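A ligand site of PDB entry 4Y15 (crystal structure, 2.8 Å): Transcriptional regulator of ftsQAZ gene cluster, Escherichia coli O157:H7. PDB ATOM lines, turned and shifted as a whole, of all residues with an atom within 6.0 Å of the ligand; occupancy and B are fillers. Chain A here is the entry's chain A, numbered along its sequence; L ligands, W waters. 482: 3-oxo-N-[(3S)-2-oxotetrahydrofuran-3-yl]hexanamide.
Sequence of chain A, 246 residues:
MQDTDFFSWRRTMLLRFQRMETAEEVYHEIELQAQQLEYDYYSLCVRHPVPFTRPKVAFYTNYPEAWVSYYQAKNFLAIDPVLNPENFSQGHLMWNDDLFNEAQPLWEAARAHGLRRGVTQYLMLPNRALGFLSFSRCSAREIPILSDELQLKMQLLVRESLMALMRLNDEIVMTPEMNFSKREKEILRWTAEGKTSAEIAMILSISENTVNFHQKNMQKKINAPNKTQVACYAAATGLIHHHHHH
The backbone NH (N) of Leu 115 lies within hydrogen-bond range of the backbone carbonyl oxygen (O) of Ala 110. The side-chain carboxylate (OD1) of Asp 80 is in hydrogen-bond range of the backbone NH (N) of Val 82, 3.0 Å away. O of Cys 45 is in hydrogen-bond range of N of Phe 132, at 2.6 Å. The side-chain hydroxyl of Tyr 71 sits at hydrogen-bond distance from the side-chain carboxylate of Asp 80, 2.7 Å away. The backbone carbonyl oxygen (O) of Ser 43 is in hydrogen-bond range of the backbone NH (N) of Ser 134 (2.9 Å). The side-chain hydroxyl (OG1) of Thr 61 lies within hydrogen-bond range of the backbone NH (N) of Tyr 63. The side-chain hydroxyl (OG) of Ser 134 is in hydrogen-bond range of the side-chain hydroxyl (OG1) of Thr 120, 2.8 Å away. The indole nitrogen (NE1) of Trp 95 lies within hydrogen-bond range of the side-chain hydroxyl (OG1) of Thr 120.
OH of Tyr 63 sits at hydrogen-bond distance from O9 of the ligand, at 3.4 Å. The side-chain hydroxyl of Ser 43 is in hydrogen-bond range of an oxygen (O12) of the ligand, at 2.5 Å. The indole nitrogen of Trp 67 sits at hydrogen-bond distance from an oxygen (O6) of the ligand, at 2.9 Å. OD2 of Asp 80 lies within hydrogen-bond range of N7 of the ligand (3.0 Å).
Residues that only touch the ligand: Trp 95 (3.2 Å), Tyr 71 (3.5 Å), Ser 134 (3.5 Å), Cys 45 (3.8 Å), Phe 59 (3.8 Å), Leu 115 (3.8 Å), Leu 106 (3.8 Å), Leu 83 (3.9 Å) and Val 82 (3.96 Å). Of the 22 residues printed, 13 come within 4 Å of the ligand. The nearest printed residue that does not touch the ligand is Thr 61 (4.1 Å).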
ATOM      1  N   SER A  43     -14.862  28.323 -17.364  1.00  0.00           N
ATOM      2  CA  SER A  43     -15.787  29.364 -17.741  1.00  0.00           C
ATOM      3  C   SER A  43     -17.145  29.052 -17.155  1.00  0.00           C
ATOM      4  O   SER A  43     -17.697  27.978 -17.414  1.00  0.00           O
ATOM      5  CB  SER A  43     -15.868  29.491 -19.265  1.00  0.00           C
ATOM      6  OG  SER A  43     -16.852  30.441 -19.654  1.00  0.00           O
ATOM      7  N   LEU A  44     -17.680  29.979 -16.358  1.00  0.00           N
ATOM      8  CA  LEU A  44     -18.958  29.756 -15.705  1.00  0.00           C
ATOM      9  C   LEU A  44     -19.998  30.725 -16.253  1.00  0.00           C
ATOM     10  O   LEU A  44     -19.855  31.931 -16.098  1.00  0.00           O
ATOM     11  CB  LEU A  44     -18.834  29.930 -14.191  1.00  0.00           C
ATOM     12  CG  LEU A  44     -20.093  29.576 -13.385  1.00  0.00           C
ATOM     13  CD1 LEU A  44     -20.565  28.158 -13.706  1.00  0.00           C
ATOM     14  CD2 LEU A  44     -19.858  29.737 -11.899  1.00  0.00           C
ATOM     15  N   CYS A  45     -21.018  30.178 -16.886  1.00  0.00           N
ATOM     16  CA  CYS A  45     -22.000  30.967 -17.623  1.00  0.00           C
ATOM     17  C   CYS A  45     -23.402  30.667 -17.121  1.00  0.00           C
ATOM     18  O   CYS A  45     -23.720  29.528 -16.794  1.00  0.00           O
ATOM     19  CB  CYS A  45     -21.888  30.672 -19.118  1.00  0.00           C
ATOM     20  SG  CYS A  45     -22.810  31.814 -20.161  1.00  0.00           S
ATOM     21  N   PHE A  59     -21.444  35.777 -17.412  1.00  0.00           N
ATOM     22  CA  PHE A  59     -20.421  34.754 -17.253  1.00  0.00           C
ATOM     23  C   PHE A  59     -19.180  35.290 -16.545  1.00  0.00           C
ATOM     24  O   PHE A  59     -18.991  36.499 -16.425  1.00  0.00           O
ATOM     25  CB  PHE A  59     -20.024  34.134 -18.599  1.00  0.00           C
ATOM     26  CG  PHE A  59     -19.391  35.111 -19.558  1.00  0.00           C
ATOM     27  CD1 PHE A  59     -18.070  35.495 -19.416  1.00  0.00           C
ATOM     28  CD2 PHE A  59     -20.114  35.613 -20.622  1.00  0.00           C
ATOM     29  CE1 PHE A  59     -17.487  36.380 -20.306  1.00  0.00           C
ATOM     30  CE2 PHE A  59     -19.540  36.510 -21.518  1.00  0.00           C
ATOM     31  CZ  PHE A  59     -18.215  36.884 -21.358  1.00  0.00           C
ATOM     32  N   THR A  61     -14.915  34.016 -16.296  1.00  0.00           N
ATOM     33  CA  THR A  61     -13.921  33.064 -16.798  1.00  0.00           C
ATOM     34  C   THR A  61     -12.498  33.563 -16.651  1.00  0.00           C
ATOM     35  O   THR A  61     -12.258  34.769 -16.571  1.00  0.00           O
ATOM     36  CB  THR A  61     -14.183  32.751 -18.280  1.00  0.00           C
ATOM     37  OG1 THR A  61     -13.217  31.784 -18.737  1.00  0.00           O
ATOM     38  CG2 THR A  61     -14.068  34.013 -19.126  1.00  0.00           C
ATOM     39  N   TYR A  63     -10.428  32.759 -19.057  1.00  0.00           N
ATOM     40  CA  TYR A  63      -9.987  32.761 -20.438  1.00  0.00           C
ATOM     41  C   TYR A  63      -9.074  33.956 -20.717  1.00  0.00           C
ATOM     42  O   TYR A  63      -9.220  35.006 -20.081  1.00  0.00           O
ATOM     43  CB  TYR A  63     -11.185  32.802 -21.399  1.00  0.00           C
ATOM     44  CG  TYR A  63     -11.857  31.472 -21.686  1.00  0.00           C
ATOM     45  CD1 TYR A  63     -11.152  30.281 -21.655  1.00  0.00           C
ATOM     46  CD2 TYR A  63     -13.210  31.421 -22.009  1.00  0.00           C
ATOM     47  CE1 TYR A  63     -11.771  29.072 -21.923  1.00  0.00           C
ATOM     48  CE2 TYR A  63     -13.835  30.218 -22.288  1.00  0.00           C
ATOM     49  CZ  TYR A  63     -13.116  29.050 -22.246  1.00  0.00           C
ATOM     50  OH  TYR A  63     -13.738  27.849 -22.508  1.00  0.00           O
ATOM     51  N   TRP A  67      -9.209  36.307 -26.290  1.00  0.00           N
ATOM     52  CA  TRP A  67     -10.265  35.407 -26.754  1.00  0.00           C
ATOM     53  C   TRP A  67     -11.643  35.842 -26.296  1.00  0.00           C
ATOM     54  O   TRP A  67     -12.592  35.827 -27.078  1.00  0.00           O
ATOM     55  CB  TRP A  67      -9.988  33.975 -26.273  1.00  0.00           C
ATOM     56  CG  TRP A  67     -11.134  33.035 -26.482  1.00  0.00           C
ATOM     57  CD1 TRP A  67     -11.748  32.274 -25.531  1.00  0.00           C
ATOM     58  CD2 TRP A  67     -11.818  32.755 -27.717  1.00  0.00           C
ATOM     59  NE1 TRP A  67     -12.765  31.540 -26.088  1.00  0.00           N
ATOM     60  CE2 TRP A  67     -12.831  31.821 -27.434  1.00  0.00           C
ATOM     61  CE3 TRP A  67     -11.668  33.205 -29.033  1.00  0.00           C
ATOM     62  CZ2 TRP A  67     -13.684  31.326 -28.407  1.00  0.00           C
ATOM     63  CZ3 TRP A  67     -12.524  32.718 -30.001  1.00  0.00           C
ATOM     64  CH2 TRP A  67     -13.517  31.783 -29.686  1.00  0.00           C
ATOM     65  N   VAL A  68     -11.758  36.239 -25.036  1.00  0.00           N
ATOM     66  CA  VAL A  68     -13.027  36.723 -24.491  1.00  0.00           C
ATOM     67  C   VAL A  68     -13.539  37.913 -25.302  1.00  0.00           C
ATOM     68  O   VAL A  68     -14.715  37.973 -25.664  1.00  0.00           O
ATOM     69  CB  VAL A  68     -12.887  37.124 -23.004  1.00  0.00           C
ATOM     70  CG1 VAL A  68     -14.203  37.655 -22.463  1.00  0.00           C
ATOM     71  CG2 VAL A  68     -12.435  35.926 -22.179  1.00  0.00           C
ATOM     72  N   TYR A  71     -14.704  36.727 -28.726  1.00  0.00           N
ATOM     73  CA  TYR A  71     -15.944  35.963 -28.551  1.00  0.00           C
ATOM     74  C   TYR A  71     -17.162  36.884 -28.446  1.00  0.00           C
ATOM     75  O   TYR A  71     -18.180  36.657 -29.102  1.00  0.00           O
ATOM     76  CB  TYR A  71     -15.843  35.099 -27.297  1.00  0.00           C
ATOM     77  CG  TYR A  71     -17.009  34.176 -27.067  1.00  0.00           C
ATOM     78  CD1 TYR A  71     -18.147  34.623 -26.405  1.00  0.00           C
ATOM     79  CD2 TYR A  71     -16.980  32.854 -27.496  1.00  0.00           C
ATOM     80  CE1 TYR A  71     -19.224  33.790 -26.181  1.00  0.00           C
ATOM     81  CE2 TYR A  71     -18.057  32.007 -27.269  1.00  0.00           C
ATOM     82  CZ  TYR A  71     -19.172  32.482 -26.617  1.00  0.00           C
ATOM     83  OH  TYR A  71     -20.240  31.650 -26.389  1.00  0.00           O
ATOM     84  N   LEU A  77     -22.231  34.098 -28.144  1.00  0.00           N
ATOM     85  CA  LEU A  77     -23.194  33.571 -27.184  1.00  0.00           C
ATOM     86  C   LEU A  77     -24.459  33.094 -27.879  1.00  0.00           C
ATOM     87  O   LEU A  77     -25.080  32.109 -27.473  1.00  0.00           O
ATOM     88  CB  LEU A  77     -23.574  34.605 -26.110  1.00  0.00           C
ATOM     89  CG  LEU A  77     -22.624  34.822 -24.945  1.00  0.00           C
ATOM     90  CD1 LEU A  77     -23.056  36.043 -24.147  1.00  0.00           C
ATOM     91  CD2 LEU A  77     -22.575  33.584 -24.056  1.00  0.00           C
ATOM     92  N   ASP A  80     -23.558  29.500 -29.506  1.00  0.00           N
ATOM     93  CA  ASP A  80     -22.654  28.545 -28.871  1.00  0.00           C
ATOM     94  C   ASP A  80     -23.384  27.242 -28.527  1.00  0.00           C
ATOM     95  O   ASP A  80     -24.332  27.253 -27.742  1.00  0.00           O
ATOM     96  CB  ASP A  80     -22.036  29.157 -27.605  1.00  0.00           C
ATOM     97  CG  ASP A  80     -20.793  28.414 -27.143  1.00  0.00           C
ATOM     98  OD1 ASP A  80     -20.615  27.237 -27.528  1.00  0.00           O
ATOM     99  OD2 ASP A  80     -19.984  29.007 -26.383  1.00  0.00           O
ATOM    100  N   VAL A  82     -22.250  24.794 -26.832  1.00  0.00           N
ATOM    101  CA  VAL A  82     -21.911  24.431 -25.464  1.00  0.00           C
ATOM    102  C   VAL A  82     -22.945  24.983 -24.478  1.00  0.00           C
ATOM    103  O   VAL A  82     -23.060  24.503 -23.344  1.00  0.00           O
ATOM    104  CB  VAL A  82     -20.497  24.943 -25.114  1.00  0.00           C
ATOM    105  CG1 VAL A  82     -20.238  24.878 -23.616  1.00  0.00           C
ATOM    106  CG2 VAL A  82     -19.452  24.138 -25.864  1.00  0.00           C
ATOM    107  N   LEU A  83     -23.724  25.962 -24.922  1.00  0.00           N
ATOM    108  CA  LEU A  83     -24.757  26.580 -24.093  1.00  0.00           C
ATOM    109  C   LEU A  83     -26.166  26.151 -24.507  1.00  0.00           C
ATOM    110  O   LEU A  83     -27.156  26.771 -24.095  1.00  0.00           O
ATOM    111  CB  LEU A  83     -24.636  28.105 -24.166  1.00  0.00           C
ATOM    112  CG  LEU A  83     -23.260  28.688 -23.851  1.00  0.00           C
ATOM    113  CD1 LEU A  83     -23.255  30.199 -24.089  1.00  0.00           C
ATOM    114  CD2 LEU A  83     -22.849  28.398 -22.416  1.00  0.00           C
ATOM    115  N   TRP A  95     -16.583  18.142 -25.799  1.00  0.00           N
ATOM    116  CA  TRP A  95     -16.489  18.913 -27.024  1.00  0.00           C
ATOM    117  C   TRP A  95     -15.890  18.066 -28.131  1.00  0.00           C
ATOM    118  O   TRP A  95     -14.909  17.353 -27.912  1.00  0.00           O
ATOM    119  CB  TRP A  95     -15.644  20.184 -26.846  1.00  0.00           C
ATOM    120  CG  TRP A  95     -16.082  21.120 -25.736  1.00  0.00           C
ATOM    121  CD1 TRP A  95     -17.117  20.940 -24.867  1.00  0.00           C
ATOM    122  CD2 TRP A  95     -15.484  22.381 -25.408  1.00  0.00           C
ATOM    123  NE1 TRP A  95     -17.197  22.018 -24.004  1.00  0.00           N
ATOM    124  CE2 TRP A  95     -16.208  22.916 -24.323  1.00  0.00           C
ATOM    125  CE3 TRP A  95     -14.414  23.113 -25.924  1.00  0.00           C
ATOM    126  CZ2 TRP A  95     -15.894  24.139 -23.747  1.00  0.00           C
ATOM    127  CZ3 TRP A  95     -14.100  24.336 -25.347  1.00  0.00           C
ATOM    128  CH2 TRP A  95     -14.838  24.833 -24.271  1.00  0.00           C
ATOM    129  N   PHE A 100     -19.789  21.561 -33.491  1.00  0.00           N
ATOM    130  CA  PHE A 100     -19.724  22.911 -34.060  1.00  0.00           C
ATOM    131  C   PHE A 100     -19.959  22.904 -35.568  1.00  0.00           C
ATOM    132  O   PHE A 100     -19.482  23.792 -36.279  1.00  0.00           O
ATOM    133  CB  PHE A 100     -18.372  23.541 -33.754  1.00  0.00           C
ATOM    134  CG  PHE A 100     -18.053  23.638 -32.293  1.00  0.00           C
ATOM    135  CD1 PHE A 100     -18.401  24.759 -31.560  1.00  0.00           C
ATOM    136  CD2 PHE A 100     -17.404  22.600 -31.647  1.00  0.00           C
ATOM    137  CE1 PHE A 100     -18.119  24.841 -30.213  1.00  0.00           C
ATOM    138  CE2 PHE A 100     -17.110  22.676 -30.302  1.00  0.00           C
ATOM    139  CZ  PHE A 100     -17.474  23.800 -29.584  1.00  0.00           C
ATOM    140  N   LEU A 106     -17.101  29.773 -34.860  1.00  0.00           N
ATOM    141  CA  LEU A 106     -16.728  29.786 -33.449  1.00  0.00           C
ATOM    142  C   LEU A 106     -15.569  28.830 -33.193  1.00  0.00           C
ATOM    143  O   LEU A 106     -14.579  29.188 -32.561  1.00  0.00           O
ATOM    144  CB  LEU A 106     -17.911  29.421 -32.561  1.00  0.00           C
ATOM    145  CG  LEU A 106     -17.576  29.058 -31.102  1.00  0.00           C
ATOM    146  CD1 LEU A 106     -16.940  30.236 -30.395  1.00  0.00           C
ATOM    147  CD2 LEU A 106     -18.808  28.588 -30.353  1.00  0.00           C
ATOM    148  N   TRP A 107     -15.703  27.613 -33.708  1.00  0.00           N
ATOM    149  CA  TRP A 107     -14.722  26.562 -33.492  1.00  0.00           C
ATOM    150  C   TRP A 107     -13.360  26.963 -34.058  1.00  0.00           C
ATOM    151  O   TRP A 107     -12.326  26.739 -33.437  1.00  0.00           O
ATOM    152  CB  TRP A 107     -15.205  25.244 -34.105  1.00  0.00           C
ATOM    153  CG  TRP A 107     -14.299  24.079 -33.858  1.00  0.00           C
ATOM    154  CD1 TRP A 107     -13.701  23.282 -34.794  1.00  0.00           C
ATOM    155  CD2 TRP A 107     -13.892  23.560 -32.578  1.00  0.00           C
ATOM    156  NE1 TRP A 107     -12.948  22.308 -34.183  1.00  0.00           N
ATOM    157  CE2 TRP A 107     -13.053  22.465 -32.821  1.00  0.00           C
ATOM    158  CE3 TRP A 107     -14.160  23.931 -31.256  1.00  0.00           C
ATOM    159  CZ2 TRP A 107     -12.471  21.726 -31.790  1.00  0.00           C
ATOM    160  CZ3 TRP A 107     -13.576  23.199 -30.232  1.00  0.00           C
ATOM    161  CH2 TRP A 107     -12.747  22.105 -30.504  1.00  0.00           C
ATOM    162  N   ALA A 110     -11.810  29.674 -32.001  1.00  0.00           N
ATOM    163  CA  ALA A 110     -11.406  29.091 -30.720  1.00  0.00           C
ATOM    164  C   ALA A 110     -10.080  28.355 -30.829  1.00  0.00           C
ATOM    165  O   ALA A 110      -9.197  28.534 -29.991  1.00  0.00           O
ATOM    166  CB  ALA A 110     -12.491  28.156 -30.211  1.00  0.00           C
ATOM    167  N   LEU A 115      -7.627  26.933 -27.898  1.00  0.00           N
ATOM    168  CA  LEU A 115      -8.548  26.023 -27.213  1.00  0.00           C
ATOM    169  C   LEU A 115      -8.719  24.718 -27.980  1.00  0.00           C
ATOM    170  O   LEU A 115      -9.485  24.631 -28.944  1.00  0.00           O
ATOM    171  CB  LEU A 115      -9.895  26.703 -27.011  1.00  0.00           C
ATOM    172  CG  LEU A 115      -9.833  27.991 -26.188  1.00  0.00           C
ATOM    173  CD1 LEU A 115     -11.196  28.638 -26.120  1.00  0.00           C
ATOM    174  CD2 LEU A 115      -9.339  27.664 -24.782  1.00  0.00           C
ATOM    175  N   THR A 120     -18.137  20.394 -20.872  1.00  0.00           N
ATOM    176  CA  THR A 120     -19.101  21.261 -20.205  1.00  0.00           C
ATOM    177  C   THR A 120     -20.141  20.504 -19.385  1.00  0.00           C
ATOM    178  O   THR A 120     -20.629  19.449 -19.805  1.00  0.00           O
ATOM    179  CB  THR A 120     -19.819  22.160 -21.218  1.00  0.00           C
ATOM    180  OG1 THR A 120     -18.841  22.916 -21.941  1.00  0.00           O
ATOM    181  CG2 THR A 120     -20.792  23.109 -20.529  1.00  0.00           C
ATOM    182  N   PHE A 132     -23.832  26.924 -16.649  1.00  0.00           N
ATOM    183  CA  PHE A 132     -22.920  26.127 -17.474  1.00  0.00           C
ATOM    184  C   PHE A 132     -21.477  26.267 -17.001  1.00  0.00           C
ATOM    185  O   PHE A 132     -20.919  27.362 -17.000  1.00  0.00           O
ATOM    186  CB  PHE A 132     -22.999  26.560 -18.941  1.00  0.00           C
ATOM    187  CG  PHE A 132     -24.359  26.394 -19.553  1.00  0.00           C
ATOM    188  CD1 PHE A 132     -24.644  25.300 -20.346  1.00  0.00           C
ATOM    189  CD2 PHE A 132     -25.348  27.344 -19.352  1.00  0.00           C
ATOM    190  CE1 PHE A 132     -25.889  25.146 -20.925  1.00  0.00           C
ATOM    191  CE2 PHE A 132     -26.595  27.198 -19.926  1.00  0.00           C
ATOM    192  CZ  PHE A 132     -26.873  26.099 -20.707  1.00  0.00           C
ATOM    193  N   SER A 134     -17.724  25.136 -18.007  1.00  0.00           N
ATOM    194  CA  SER A 134     -16.866  24.582 -19.038  1.00  0.00           C
ATOM    195  C   SER A 134     -15.434  24.521 -18.556  1.00  0.00           C
ATOM    196  O   SER A 134     -14.961  25.457 -17.907  1.00  0.00           O
ATOM    197  CB  SER A 134     -16.935  25.422 -20.313  1.00  0.00           C
ATOM    198  OG  SER A 134     -18.227  25.387 -20.891  1.00  0.00           O
HETATM  199  C15 482 L   1     -16.912  32.806 -21.836  1.00  0.00           C
HETATM  200  C14 482 L   1     -17.302  32.358 -23.229  1.00  0.00           C
HETATM  201  C13 482 L   1     -18.735  31.859 -23.247  1.00  0.00           C
HETATM  202  C11 482 L   1     -18.866  30.579 -22.461  1.00  0.00           C
HETATM  203  O12 482 L   1     -18.754  30.601 -21.241  1.00  0.00           O
HETATM  204  C10 482 L   1     -19.142  29.258 -23.154  1.00  0.00           C
HETATM  205  C8  482 L   1     -17.827  28.599 -23.521  1.00  0.00           C
HETATM  206  O9  482 L   1     -17.070  28.215 -22.653  1.00  0.00           O
HETATM  207  N7  482 L   1     -17.489  28.425 -24.888  1.00  0.00           N
HETATM  208  C1  482 L   1     -16.281  27.816 -25.223  1.00  0.00           C
HETATM  209  C5  482 L   1     -16.509  26.760 -26.270  1.00  0.00           C
HETATM  210  C4  482 L   1     -15.714  27.165 -27.470  1.00  0.00           C
HETATM  211  C2  482 L   1     -15.419  28.776 -25.887  1.00  0.00           C
HETATM  212  O6  482 L   1     -14.785  29.659 -25.346  1.00  0.00           O
HETATM  213  OAP 482 L   1     -15.445  28.488 -27.341  1.00  0.00           O
HETATM  214  O   HOH W   1     -19.282  27.658 -19.803  1.00  0.00           O
